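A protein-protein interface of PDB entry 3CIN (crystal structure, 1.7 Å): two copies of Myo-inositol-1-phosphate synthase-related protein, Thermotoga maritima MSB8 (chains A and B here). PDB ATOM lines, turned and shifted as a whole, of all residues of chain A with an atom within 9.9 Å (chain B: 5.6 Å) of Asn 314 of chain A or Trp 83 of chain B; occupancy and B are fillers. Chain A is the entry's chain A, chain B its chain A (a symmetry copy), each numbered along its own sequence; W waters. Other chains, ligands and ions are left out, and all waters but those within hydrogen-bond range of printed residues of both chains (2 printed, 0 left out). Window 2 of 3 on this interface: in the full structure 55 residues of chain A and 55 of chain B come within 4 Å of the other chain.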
ATOM      1  N   ASN A 240      23.251  -5.717  31.627  1.00  0.00           N
ATOM      2  CA  ASN A 240      22.358  -6.239  32.680  1.00  0.00           C
ATOM      3  C   ASN A 240      22.679  -7.675  32.991  1.00  0.00           C
ATOM      4  O   ASN A 240      21.793  -8.520  33.146  1.00  0.00           O
ATOM      5  CB  ASN A 240      20.898  -6.110  32.247  1.00  0.00           C
ATOM      6  CG  ASN A 240      19.940  -6.275  33.396  1.00  0.00           C
ATOM      7  OD1 ASN A 240      20.331  -6.028  34.544  1.00  0.00           O
ATOM      8  ND2 ASN A 240      18.715  -6.692  33.120  1.00  0.00           N
ATOM      9  N   ARG A 241      23.971  -7.991  33.023  1.00  0.00           N
ATOM     10  CA  ARG A 241      24.408  -9.331  33.373  1.00  0.00           C
ATOM     11  C   ARG A 241      24.636  -9.393  34.888  1.00  0.00           C
ATOM     12  O   ARG A 241      25.362  -8.559  35.405  1.00  0.00           O
ATOM     13  CB  ARG A 241      25.703  -9.659  32.619  1.00  0.00           C
ATOM     14  CG  ARG A 241      25.387  -9.883  31.148  1.00  0.00           C
ATOM     15  CD  ARG A 241      26.659  -9.989  30.345  1.00  0.00           C
ATOM     16  NE  ARG A 241      26.371 -10.453  28.993  1.00  0.00           N
ATOM     17  CZ  ARG A 241      27.310 -10.595  28.049  1.00  0.00           C
ATOM     18  NH1 ARG A 241      28.583 -10.268  28.285  1.00  0.00           N
ATOM     19  NH2 ARG A 241      26.965 -11.034  26.852  1.00  0.00           N
ATOM     20  N   TYR A 310      29.000 -14.728  35.876  1.00  0.00           N
ATOM     21  CA  TYR A 310      27.808 -13.918  35.755  1.00  0.00           C
ATOM     22  C   TYR A 310      26.701 -14.645  35.050  1.00  0.00           C
ATOM     23  O   TYR A 310      26.924 -15.610  34.334  1.00  0.00           O
ATOM     24  CB  TYR A 310      28.132 -12.599  35.059  1.00  0.00           C
ATOM     25  CG  TYR A 310      28.729 -12.738  33.671  1.00  0.00           C
ATOM     26  CD1 TYR A 310      30.116 -12.812  33.472  1.00  0.00           C
ATOM     27  CD2 TYR A 310      27.894 -12.732  32.547  1.00  0.00           C
ATOM     28  CE1 TYR A 310      30.591 -12.968  32.210  1.00  0.00           C
ATOM     29  CE2 TYR A 310      28.403 -12.835  31.272  1.00  0.00           C
ATOM     30  CZ  TYR A 310      29.758 -12.929  31.123  1.00  0.00           C
ATOM     31  OH  TYR A 310      30.259 -13.067  29.842  1.00  0.00           O
ATOM     32  N   VAL A 311      25.474 -14.177  35.262  1.00  0.00           N
ATOM     33  CA  VAL A 311      24.317 -14.781  34.652  1.00  0.00           C
ATOM     34  C   VAL A 311      23.895 -13.954  33.440  1.00  0.00           C
ATOM     35  O   VAL A 311      23.750 -12.757  33.550  1.00  0.00           O
ATOM     36  CB  VAL A 311      23.114 -14.796  35.628  1.00  0.00           C
ATOM     37  CG1 VAL A 311      21.885 -15.404  34.987  1.00  0.00           C
ATOM     38  CG2 VAL A 311      23.507 -15.599  36.877  1.00  0.00           C
ATOM     39  N   SER A 312      23.653 -14.636  32.335  1.00  0.00           N
ATOM     40  CA  SER A 312      23.280 -13.991  31.096  1.00  0.00           C
ATOM     41  C   SER A 312      21.793 -14.318  30.877  1.00  0.00           C
ATOM     42  O   SER A 312      21.040 -14.547  31.843  1.00  0.00           O
ATOM     43  CB  SER A 312      24.220 -14.502  29.982  1.00  0.00           C
ATOM     44  OG  SER A 312      23.771 -14.289  28.661  1.00  0.00           O
ATOM     45  N   PHE A 313      21.335 -14.311  29.638  1.00  0.00           N
ATOM     46  CA  PHE A 313      19.937 -14.560  29.310  1.00  0.00           C
ATOM     47  C   PHE A 313      19.518 -16.008  29.490  1.00  0.00           C
ATOM     48  O   PHE A 313      20.304 -16.952  29.298  1.00  0.00           O
ATOM     49  CB  PHE A 313      19.763 -14.126  27.848  1.00  0.00           C
ATOM     50  CG  PHE A 313      18.362 -14.105  27.326  1.00  0.00           C
ATOM     51  CD1 PHE A 313      17.446 -13.184  27.809  1.00  0.00           C
ATOM     52  CD2 PHE A 313      17.966 -14.951  26.290  1.00  0.00           C
ATOM     53  CE1 PHE A 313      16.195 -13.158  27.278  1.00  0.00           C
ATOM     54  CE2 PHE A 313      16.733 -14.889  25.761  1.00  0.00           C
ATOM     55  CZ  PHE A 313      15.844 -13.987  26.277  1.00  0.00           C
ATOM     56  N   ASN A 314      18.237 -16.210  29.807  1.00  0.00           N
ATOM     57  CA  ASN A 314      17.643 -17.529  29.873  1.00  0.00           C
ATOM     58  C   ASN A 314      18.374 -18.431  30.878  1.00  0.00           C
ATOM     59  O   ASN A 314      18.418 -19.638  30.659  1.00  0.00           O
ATOM     60  CB  ASN A 314      17.575 -18.228  28.499  1.00  0.00           C
ATOM     61  CG  ASN A 314      16.469 -19.296  28.417  1.00  0.00           C
ATOM     62  OD1 ASN A 314      15.441 -19.186  29.064  1.00  0.00           O
ATOM     63  ND2 ASN A 314      16.702 -20.343  27.622  1.00  0.00           N
ATOM     64  N   GLY A 315      18.935 -17.830  31.921  1.00  0.00           N
ATOM     65  CA  GLY A 315      19.492 -18.577  33.009  1.00  0.00           C
ATOM     66  C   GLY A 315      20.900 -19.049  32.727  1.00  0.00           C
ATOM     67  O   GLY A 315      21.505 -19.730  33.540  1.00  0.00           O
ATOM     68  N   ALA A 316      21.426 -18.713  31.560  1.00  0.00           N
ATOM     69  CA  ALA A 316      22.808 -19.070  31.214  1.00  0.00           C
ATOM     70  C   ALA A 316      23.860 -18.430  32.139  1.00  0.00           C
ATOM     71  O   ALA A 316      23.692 -17.314  32.569  1.00  0.00           O
ATOM     72  CB  ALA A 316      23.056 -18.636  29.747  1.00  0.00           C
ATOM     73  N   THR A 317      24.965 -19.150  32.420  1.00  0.00           N
ATOM     74  CA  THR A 317      26.030 -18.677  33.277  1.00  0.00           C
ATOM     75  C   THR A 317      27.387 -18.729  32.502  1.00  0.00           C
ATOM     76  O   THR A 317      27.710 -19.743  31.885  1.00  0.00           O
ATOM     77  CB  THR A 317      26.127 -19.550  34.554  1.00  0.00           C
ATOM     78  OG1 THR A 317      24.927 -19.371  35.337  1.00  0.00           O
ATOM     79  CG2 THR A 317      27.288 -19.146  35.412  1.00  0.00           C
ATOM     80  N   ASP A 318      28.063 -17.595  32.511  1.00  0.00           N
ATOM     81  CA  ASP A 318      29.311 -17.361  31.763  1.00  0.00           C
ATOM     82  C   ASP A 318      30.421 -17.083  32.768  1.00  0.00           C
ATOM     83  O   ASP A 318      30.161 -16.714  33.905  1.00  0.00           O
ATOM     84  CB  ASP A 318      29.189 -16.180  30.832  1.00  0.00           C
ATOM     85  CG  ASP A 318      28.194 -16.402  29.661  1.00  0.00           C
ATOM     86  OD1 ASP A 318      27.761 -17.523  29.389  1.00  0.00           O
ATOM     87  OD2 ASP A 318      27.906 -15.412  28.950  1.00  0.00           O
ATOM     88  N   TYR B  23      19.460 -21.962  16.808  1.00  0.00           N
ATOM     89  CA  TYR B  23      19.803 -21.790  18.213  1.00  0.00           C
ATOM     90  C   TYR B  23      19.495 -20.406  18.724  1.00  0.00           C
ATOM     91  O   TYR B  23      18.825 -20.282  19.760  1.00  0.00           O
ATOM     92  CB  TYR B  23      21.279 -22.091  18.446  1.00  0.00           C
ATOM     93  CG  TYR B  23      21.514 -23.002  19.609  1.00  0.00           C
ATOM     94  CD1 TYR B  23      20.980 -22.717  20.859  1.00  0.00           C
ATOM     95  CD2 TYR B  23      22.310 -24.138  19.475  1.00  0.00           C
ATOM     96  CE1 TYR B  23      21.225 -23.566  21.964  1.00  0.00           C
ATOM     97  CE2 TYR B  23      22.527 -24.979  20.528  1.00  0.00           C
ATOM     98  CZ  TYR B  23      22.012 -24.688  21.780  1.00  0.00           C
ATOM     99  OH  TYR B  23      22.254 -25.543  22.855  1.00  0.00           O
ATOM    100  N   SER B  26      15.683 -19.799  18.697  1.00  0.00           N
ATOM    101  CA  SER B  26      14.985 -20.604  19.623  1.00  0.00           C
ATOM    102  C   SER B  26      15.277 -20.162  21.076  1.00  0.00           C
ATOM    103  O   SER B  26      14.427 -20.260  21.924  1.00  0.00           O
ATOM    104  CB  SER B  26      15.332 -22.063  19.390  1.00  0.00           C
ATOM    105  OG  SER B  26      14.882 -22.494  18.121  1.00  0.00           O
ATOM    106  N   THR B  27      16.471 -19.649  21.341  1.00  0.00           N
ATOM    107  CA  THR B  27      16.785 -19.143  22.675  1.00  0.00           C
ATOM    108  C   THR B  27      16.005 -17.839  22.919  1.00  0.00           C
ATOM    109  O   THR B  27      15.486 -17.639  24.024  1.00  0.00           O
ATOM    110  CB  THR B  27      18.255 -18.895  22.793  1.00  0.00           C
ATOM    111  OG1 THR B  27      18.923 -20.140  22.575  1.00  0.00           O
ATOM    112  CG2 THR B  27      18.613 -18.369  24.184  1.00  0.00           C
ATOM    113  N   ALA B  30      12.420 -18.969  23.622  1.00  0.00           N
ATOM    114  CA  ALA B  30      12.262 -19.694  24.894  1.00  0.00           C
ATOM    115  C   ALA B  30      12.468 -18.728  26.074  1.00  0.00           C
ATOM    116  O   ALA B  30      11.750 -18.788  27.097  1.00  0.00           O
ATOM    117  CB  ALA B  30      13.252 -20.804  24.938  1.00  0.00           C
ATOM    118  N   GLY B  31      13.469 -17.870  25.940  1.00  0.00           N
ATOM    119  CA  GLY B  31      13.759 -16.860  26.959  1.00  0.00           C
ATOM    120  C   GLY B  31      12.591 -15.903  27.121  1.00  0.00           C
ATOM    121  O   GLY B  31      12.181 -15.565  28.249  1.00  0.00           O
ATOM    122  N   LYS B  34       9.735 -17.433  29.080  1.00  0.00           N
ATOM    123  CA  LYS B  34       9.989 -17.388  30.523  1.00  0.00           C
ATOM    124  C   LYS B  34       9.844 -15.995  31.072  1.00  0.00           C
ATOM    125  O   LYS B  34       9.342 -15.840  32.173  1.00  0.00           O
ATOM    126  CB  LYS B  34      11.370 -17.933  30.887  1.00  0.00           C
ATOM    127  CG  LYS B  34      11.622 -19.340  30.380  1.00  0.00           C
ATOM    128  CD  LYS B  34      11.525 -20.411  31.449  1.00  0.00           C
ATOM    129  CE  LYS B  34      12.628 -21.452  31.250  1.00  0.00           C
ATOM    130  NZ  LYS B  34      13.936 -20.805  30.863  1.00  0.00           N
ATOM    131  N   ILE B  40      11.741 -15.986  34.990  1.00  0.00           N
ATOM    132  CA  ILE B  40      13.098 -15.481  35.116  1.00  0.00           C
ATOM    133  C   ILE B  40      13.137 -13.969  35.070  1.00  0.00           C
ATOM    134  O   ILE B  40      12.251 -13.348  34.499  1.00  0.00           O
ATOM    135  CB  ILE B  40      14.033 -15.975  33.971  1.00  0.00           C
ATOM    136  CG1 ILE B  40      13.610 -15.435  32.612  1.00  0.00           C
ATOM    137  CG2 ILE B  40      14.169 -17.498  33.953  1.00  0.00           C
ATOM    138  CD1 ILE B  40      14.351 -16.064  31.416  1.00  0.00           C
ATOM    139  N   TYR B  43      17.908 -10.688  33.014  1.00  0.00           N
ATOM    140  CA  TYR B  43      19.367 -10.617  32.854  1.00  0.00           C
ATOM    141  C   TYR B  43      19.751 -10.858  31.422  1.00  0.00           C
ATOM    142  O   TYR B  43      19.090 -11.623  30.684  1.00  0.00           O
ATOM    143  CB  TYR B  43      20.072 -11.589  33.789  1.00  0.00           C
ATOM    144  CG  TYR B  43      19.682 -11.411  35.196  1.00  0.00           C
ATOM    145  CD1 TYR B  43      19.764 -10.144  35.814  1.00  0.00           C
ATOM    146  CD2 TYR B  43      19.197 -12.465  35.939  1.00  0.00           C
ATOM    147  CE1 TYR B  43      19.363  -9.970  37.107  1.00  0.00           C
ATOM    148  CE2 TYR B  43      18.798 -12.291  37.244  1.00  0.00           C
ATOM    149  CZ  TYR B  43      18.916 -11.048  37.839  1.00  0.00           C
ATOM    150  OH  TYR B  43      18.515 -10.877  39.138  1.00  0.00           O
ATOM    151  N   VAL B  79      11.658 -25.298  19.028  1.00  0.00           N
ATOM    152  CA  VAL B  79      12.274 -24.679  20.242  1.00  0.00           C
ATOM    153  C   VAL B  79      12.662 -25.743  21.301  1.00  0.00           C
ATOM    154  O   VAL B  79      13.790 -25.687  21.846  1.00  0.00           O
ATOM    155  CB  VAL B  79      11.380 -23.515  20.809  1.00  0.00           C
ATOM    156  CG1 VAL B  79      11.938 -22.993  22.113  1.00  0.00           C
ATOM    157  CG2 VAL B  79      11.304 -22.366  19.780  1.00  0.00           C
ATOM    158  N   LYS B  80      11.801 -26.748  21.553  1.00  0.00           N
ATOM    159  CA  LYS B  80      12.110 -27.801  22.527  1.00  0.00           C
ATOM    160  C   LYS B  80      13.333 -28.620  22.152  1.00  0.00           C
ATOM    161  O   LYS B  80      13.979 -29.173  23.030  1.00  0.00           O
ATOM    162  CB  LYS B  80      10.939 -28.729  22.706  1.00  0.00           C
ATOM    163  CG  LYS B  80      11.028 -29.732  23.838  1.00  0.00           C
ATOM    164  CD  LYS B  80       9.914 -30.764  23.713  1.00  0.00           C
ATOM    165  CE  LYS B  80       9.417 -31.299  25.067  1.00  0.00           C
ATOM    166  NZ  LYS B  80      10.273 -31.046  26.245  1.00  0.00           N
ATOM    167  N   GLN B  81      13.675 -28.696  20.874  1.00  0.00           N
ATOM    168  CA  GLN B  81      14.895 -29.377  20.490  1.00  0.00           C
ATOM    169  C   GLN B  81      16.094 -28.654  21.048  1.00  0.00           C
ATOM    170  O   GLN B  81      17.100 -29.281  21.277  1.00  0.00           O
ATOM    171  CB  GLN B  81      15.030 -29.485  18.967  1.00  0.00           C
ATOM    172  CG  GLN B  81      13.974 -30.374  18.313  1.00  0.00           C
ATOM    173  CD  GLN B  81      13.878 -30.172  16.794  1.00  0.00           C
ATOM    174  OE1 GLN B  81      14.846 -29.765  16.141  1.00  0.00           O
ATOM    175  NE2 GLN B  81      12.690 -30.448  16.232  1.00  0.00           N
ATOM    176  N   TYR B  82      16.014 -27.329  21.224  1.00  0.00           N
ATOM    177  CA  TYR B  82      17.143 -26.561  21.773  1.00  0.00           C
ATOM    178  C   TYR B  82      17.067 -26.382  23.299  1.00  0.00           C
ATOM    179  O   TYR B  82      18.103 -26.411  23.998  1.00  0.00           O
ATOM    180  CB  TYR B  82      17.239 -25.174  21.094  1.00  0.00           C
ATOM    181  CG  TYR B  82      17.547 -25.287  19.632  1.00  0.00           C
ATOM    182  CD1 TYR B  82      18.845 -25.335  19.179  1.00  0.00           C
ATOM    183  CD2 TYR B  82      16.529 -25.322  18.684  1.00  0.00           C
ATOM    184  CE1 TYR B  82      19.140 -25.468  17.841  1.00  0.00           C
ATOM    185  CE2 TYR B  82      16.816 -25.433  17.323  1.00  0.00           C
ATOM    186  CZ  TYR B  82      18.142 -25.502  16.912  1.00  0.00           C
ATOM    187  OH  TYR B  82      18.509 -25.611  15.572  1.00  0.00           O
ATOM    188  N   TRP B  83      15.838 -26.226  23.802  1.00  0.00           N
ATOM    189  CA  TRP B  83      15.556 -26.006  25.227  1.00  0.00           C
ATOM    190  C   TRP B  83      14.453 -26.916  25.677  1.00  0.00           C
ATOM    191  O   TRP B  83      13.261 -26.644  25.480  1.00  0.00           O
ATOM    192  CB  TRP B  83      15.160 -24.544  25.444  1.00  0.00           C
ATOM    193  CG  TRP B  83      16.244 -23.647  25.097  1.00  0.00           C
ATOM    194  CD1 TRP B  83      16.375 -22.936  23.949  1.00  0.00           C
ATOM    195  CD2 TRP B  83      17.398 -23.376  25.882  1.00  0.00           C
ATOM    196  NE1 TRP B  83      17.530 -22.220  23.974  1.00  0.00           N
ATOM    197  CE2 TRP B  83      18.189 -22.472  25.144  1.00  0.00           C
ATOM    198  CE3 TRP B  83      17.837 -23.790  27.145  1.00  0.00           C
ATOM    199  CZ2 TRP B  83      19.377 -21.967  25.613  1.00  0.00           C
ATOM    200  CZ3 TRP B  83      19.047 -23.280  27.620  1.00  0.00           C
ATOM    201  CH2 TRP B  83      19.798 -22.378  26.840  1.00  0.00           C
ATOM    202  N   ASN B  84      14.866 -28.042  26.255  1.00  0.00           N
ATOM    203  CA  ASN B  84      13.969 -29.148  26.544  1.00  0.00           C
ATOM    204  C   ASN B  84      12.883 -28.795  27.565  1.00  0.00           C
ATOM    205  O   ASN B  84      11.887 -29.503  27.678  1.00  0.00           O
ATOM    206  CB  ASN B  84      14.799 -30.319  27.059  1.00  0.00           C
ATOM    207  CG  ASN B  84      13.989 -31.557  27.255  1.00  0.00           C
ATOM    208  OD1 ASN B  84      13.754 -31.980  28.380  1.00  0.00           O
ATOM    209  ND2 ASN B  84      13.535 -32.138  26.161  1.00  0.00           N
ATOM    210  N   ASP B  85      13.103 -27.711  28.313  1.00  0.00           N
ATOM    211  CA  ASP B  85      12.153 -27.272  29.353  1.00  0.00           C
ATOM    212  C   ASP B  85      10.901 -26.570  28.774  1.00  0.00           C
ATOM    213  O   ASP B  85       9.863 -26.445  29.439  1.00  0.00           O
ATOM    214  CB  ASP B  85      12.870 -26.455  30.460  1.00  0.00           C
ATOM    215  CG  ASP B  85      13.711 -25.272  29.927  1.00  0.00           C
ATOM    216  OD1 ASP B  85      14.287 -25.340  28.818  1.00  0.00           O
ATOM    217  OD2 ASP B  85      13.835 -24.272  30.667  1.00  0.00           O
ATOM    218  N   VAL B  86      10.965 -26.199  27.508  1.00  0.00           N
ATOM    219  CA  VAL B  86       9.842 -25.541  26.856  1.00  0.00           C
ATOM    220  C   VAL B  86       8.845 -26.569  26.335  1.00  0.00           C
ATOM    221  O   VAL B  86       9.139 -27.276  25.378  1.00  0.00           O
ATOM    222  CB  VAL B  86      10.354 -24.706  25.686  1.00  0.00           C
ATOM    223  CG1 VAL B  86       9.166 -24.049  24.972  1.00  0.00           C
ATOM    224  CG2 VAL B  86      11.327 -23.687  26.187  1.00  0.00           C
ATOM    225  N   ASP B 300      26.945 -24.885  22.633  1.00  0.00           N
ATOM    226  CA  ASP B 300      26.627 -23.487  22.524  1.00  0.00           C
ATOM    227  C   ASP B 300      27.515 -22.585  23.405  1.00  0.00           C
ATOM    228  O   ASP B 300      27.425 -21.358  23.318  1.00  0.00           O
ATOM    229  CB  ASP B 300      25.135 -23.256  22.821  1.00  0.00           C
ATOM    230  CG  ASP B 300      24.673 -21.870  22.408  1.00  0.00           C
ATOM    231  OD1 ASP B 300      24.908 -21.411  21.269  1.00  0.00           O
ATOM    232  OD2 ASP B 300      24.068 -21.229  23.278  1.00  0.00           O
ATOM    233  N   PRO B 330      22.361 -17.516  24.071  1.00  0.00           N
ATOM    234  CA  PRO B 330      21.711 -16.627  25.073  1.00  0.00           C
ATOM    235  C   PRO B 330      22.153 -15.182  24.994  1.00  0.00           C
ATOM    236  O   PRO B 330      21.331 -14.284  25.151  1.00  0.00           O
ATOM    237  CB  PRO B 330      22.060 -17.303  26.389  1.00  0.00           C
ATOM    238  CG  PRO B 330      22.223 -18.769  25.993  1.00  0.00           C
ATOM    239  CD  PRO B 330      22.969 -18.677  24.720  1.00  0.00           C
HETATM  240  O   HOH W   1      14.031 -22.244  28.513  1.00  0.00           O
HETATM  241  O   HOH W   2      17.174 -13.529  31.384  1.00  0.00           O
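The side-chain amide oxygen (OD1) of Asn 314 of chain A is in hydrogen-bond range of the side-chain amino group (NZ) of Lys 34 of chain B (2.9 Å).
O of Tyr 23 of chain B is in hydrogen-bond range of OG1 of Thr 27 of chain B.
The indole nitrogen (NE1) of Trp 83 of chain B lies within hydrogen-bond range of the side-chain hydroxyl (OG1) of Thr 27 of chain B, 2.9 Å away.
The side-chain carboxylate (OD2) of Asp 85 of chain B lies within salt-bridge range of the side-chain amino group (NZ) of Lys 34 of chain B.
CA of Tyr 43 of chain B touches O of Asn 240 of chain A, 3.2 Å away.
Val 311 of chain A touches Tyr 43 of chain B (O to CB, 3.9 Å).
Tyr 43 of chain B touches Ser 312 of chain A (CB to O, 3.7 Å).
Phe 313 of chain A touches Thr 27 of chain B.
CA of Gly 31 of chain B touches CZ of Phe 313 of chain A (3.6 Å).
Phe 313 of chain A touches Tyr 43 of chain B (CA to O, 3.4 Å).
O of Pro 330 of chain B touches CB of Phe 313 of chain A, 3.1 Å away.
Asn 314 of chain A touches Gly 31 of chain B.
Ile 40 of chain B touches Asn 314 of chain A (CD1 to CA, 3.9 Å).
CB of Pro 330 of chain B touches CB of Ala 316 of chain A, 3.7 Å away.
Asn 314 of chain A touches four residues of chain B.
Of chain A, only Phe 313 comes within 4 Å of Thr 27 of chain B.
Of the printed residues of chain A, Gly 31 of chain B touches Phe 313 (3.6 Å) and Asn 314 (3.6 Å).
No residue of chain A comes within 4 Å of Asp 85 of chain B.
No residue of chain A comes within 4 Å of Val 86 of chain B.
Of the printed residues of chain A, Pro 330 of chain B touches Phe 313 (3.1 Å) and Ala 316 (3.7 Å).
Printed residues of chain B within 4 Å of Phe 313 of chain A: Thr 27 (3.5 Å), Gly 31 (3.6 Å), Tyr 43 (3.4 Å) and Pro 330 (3.1 Å).
Printed residues of chain A within 4 Å of Ile 40 of chain B: Asn 314 (3.9 Å).
Lys 80 of chain B touches none of the printed residues of chain A.
The nearest residue of chain A that does not touch Trp 83 of chain B is Ala 316 of chain A (5.8 Å).
The nearest printed residue of chain B that does not touch Phe 313 of chain A is Ile 40 of chain B (5.4 Å).
Hydrophobic or aromatic side chains of chain A that line the printed part of chain B: Phe 313 and Ala 316.
Along chain A the printed residues that touch a printed residue of chain B span positions 240 to 316.
Of the 18 printed residues of chain B, 7 touch a printed residue of chain A.
No position is printed for both chains.
Of the 12 pairs that touch across the chains among the printed residues, none has its exchanged pair printed and touching as well.
Water W1 lies within hydrogen-bond range of the side-chain amino group (NZ) of Lys 34 of chain B, the side-chain carboxylate (OD2) of Asp 85 of chain B and the side-chain amide nitrogen (ND2) of Asn 314 of chain A.
Water W2 lies within hydrogen-bond range of the backbone carbonyl oxygen of Tyr 43 of chain B (2.8 Å) and the backbone NH of Asn 314 of chain A (3.3 Å).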
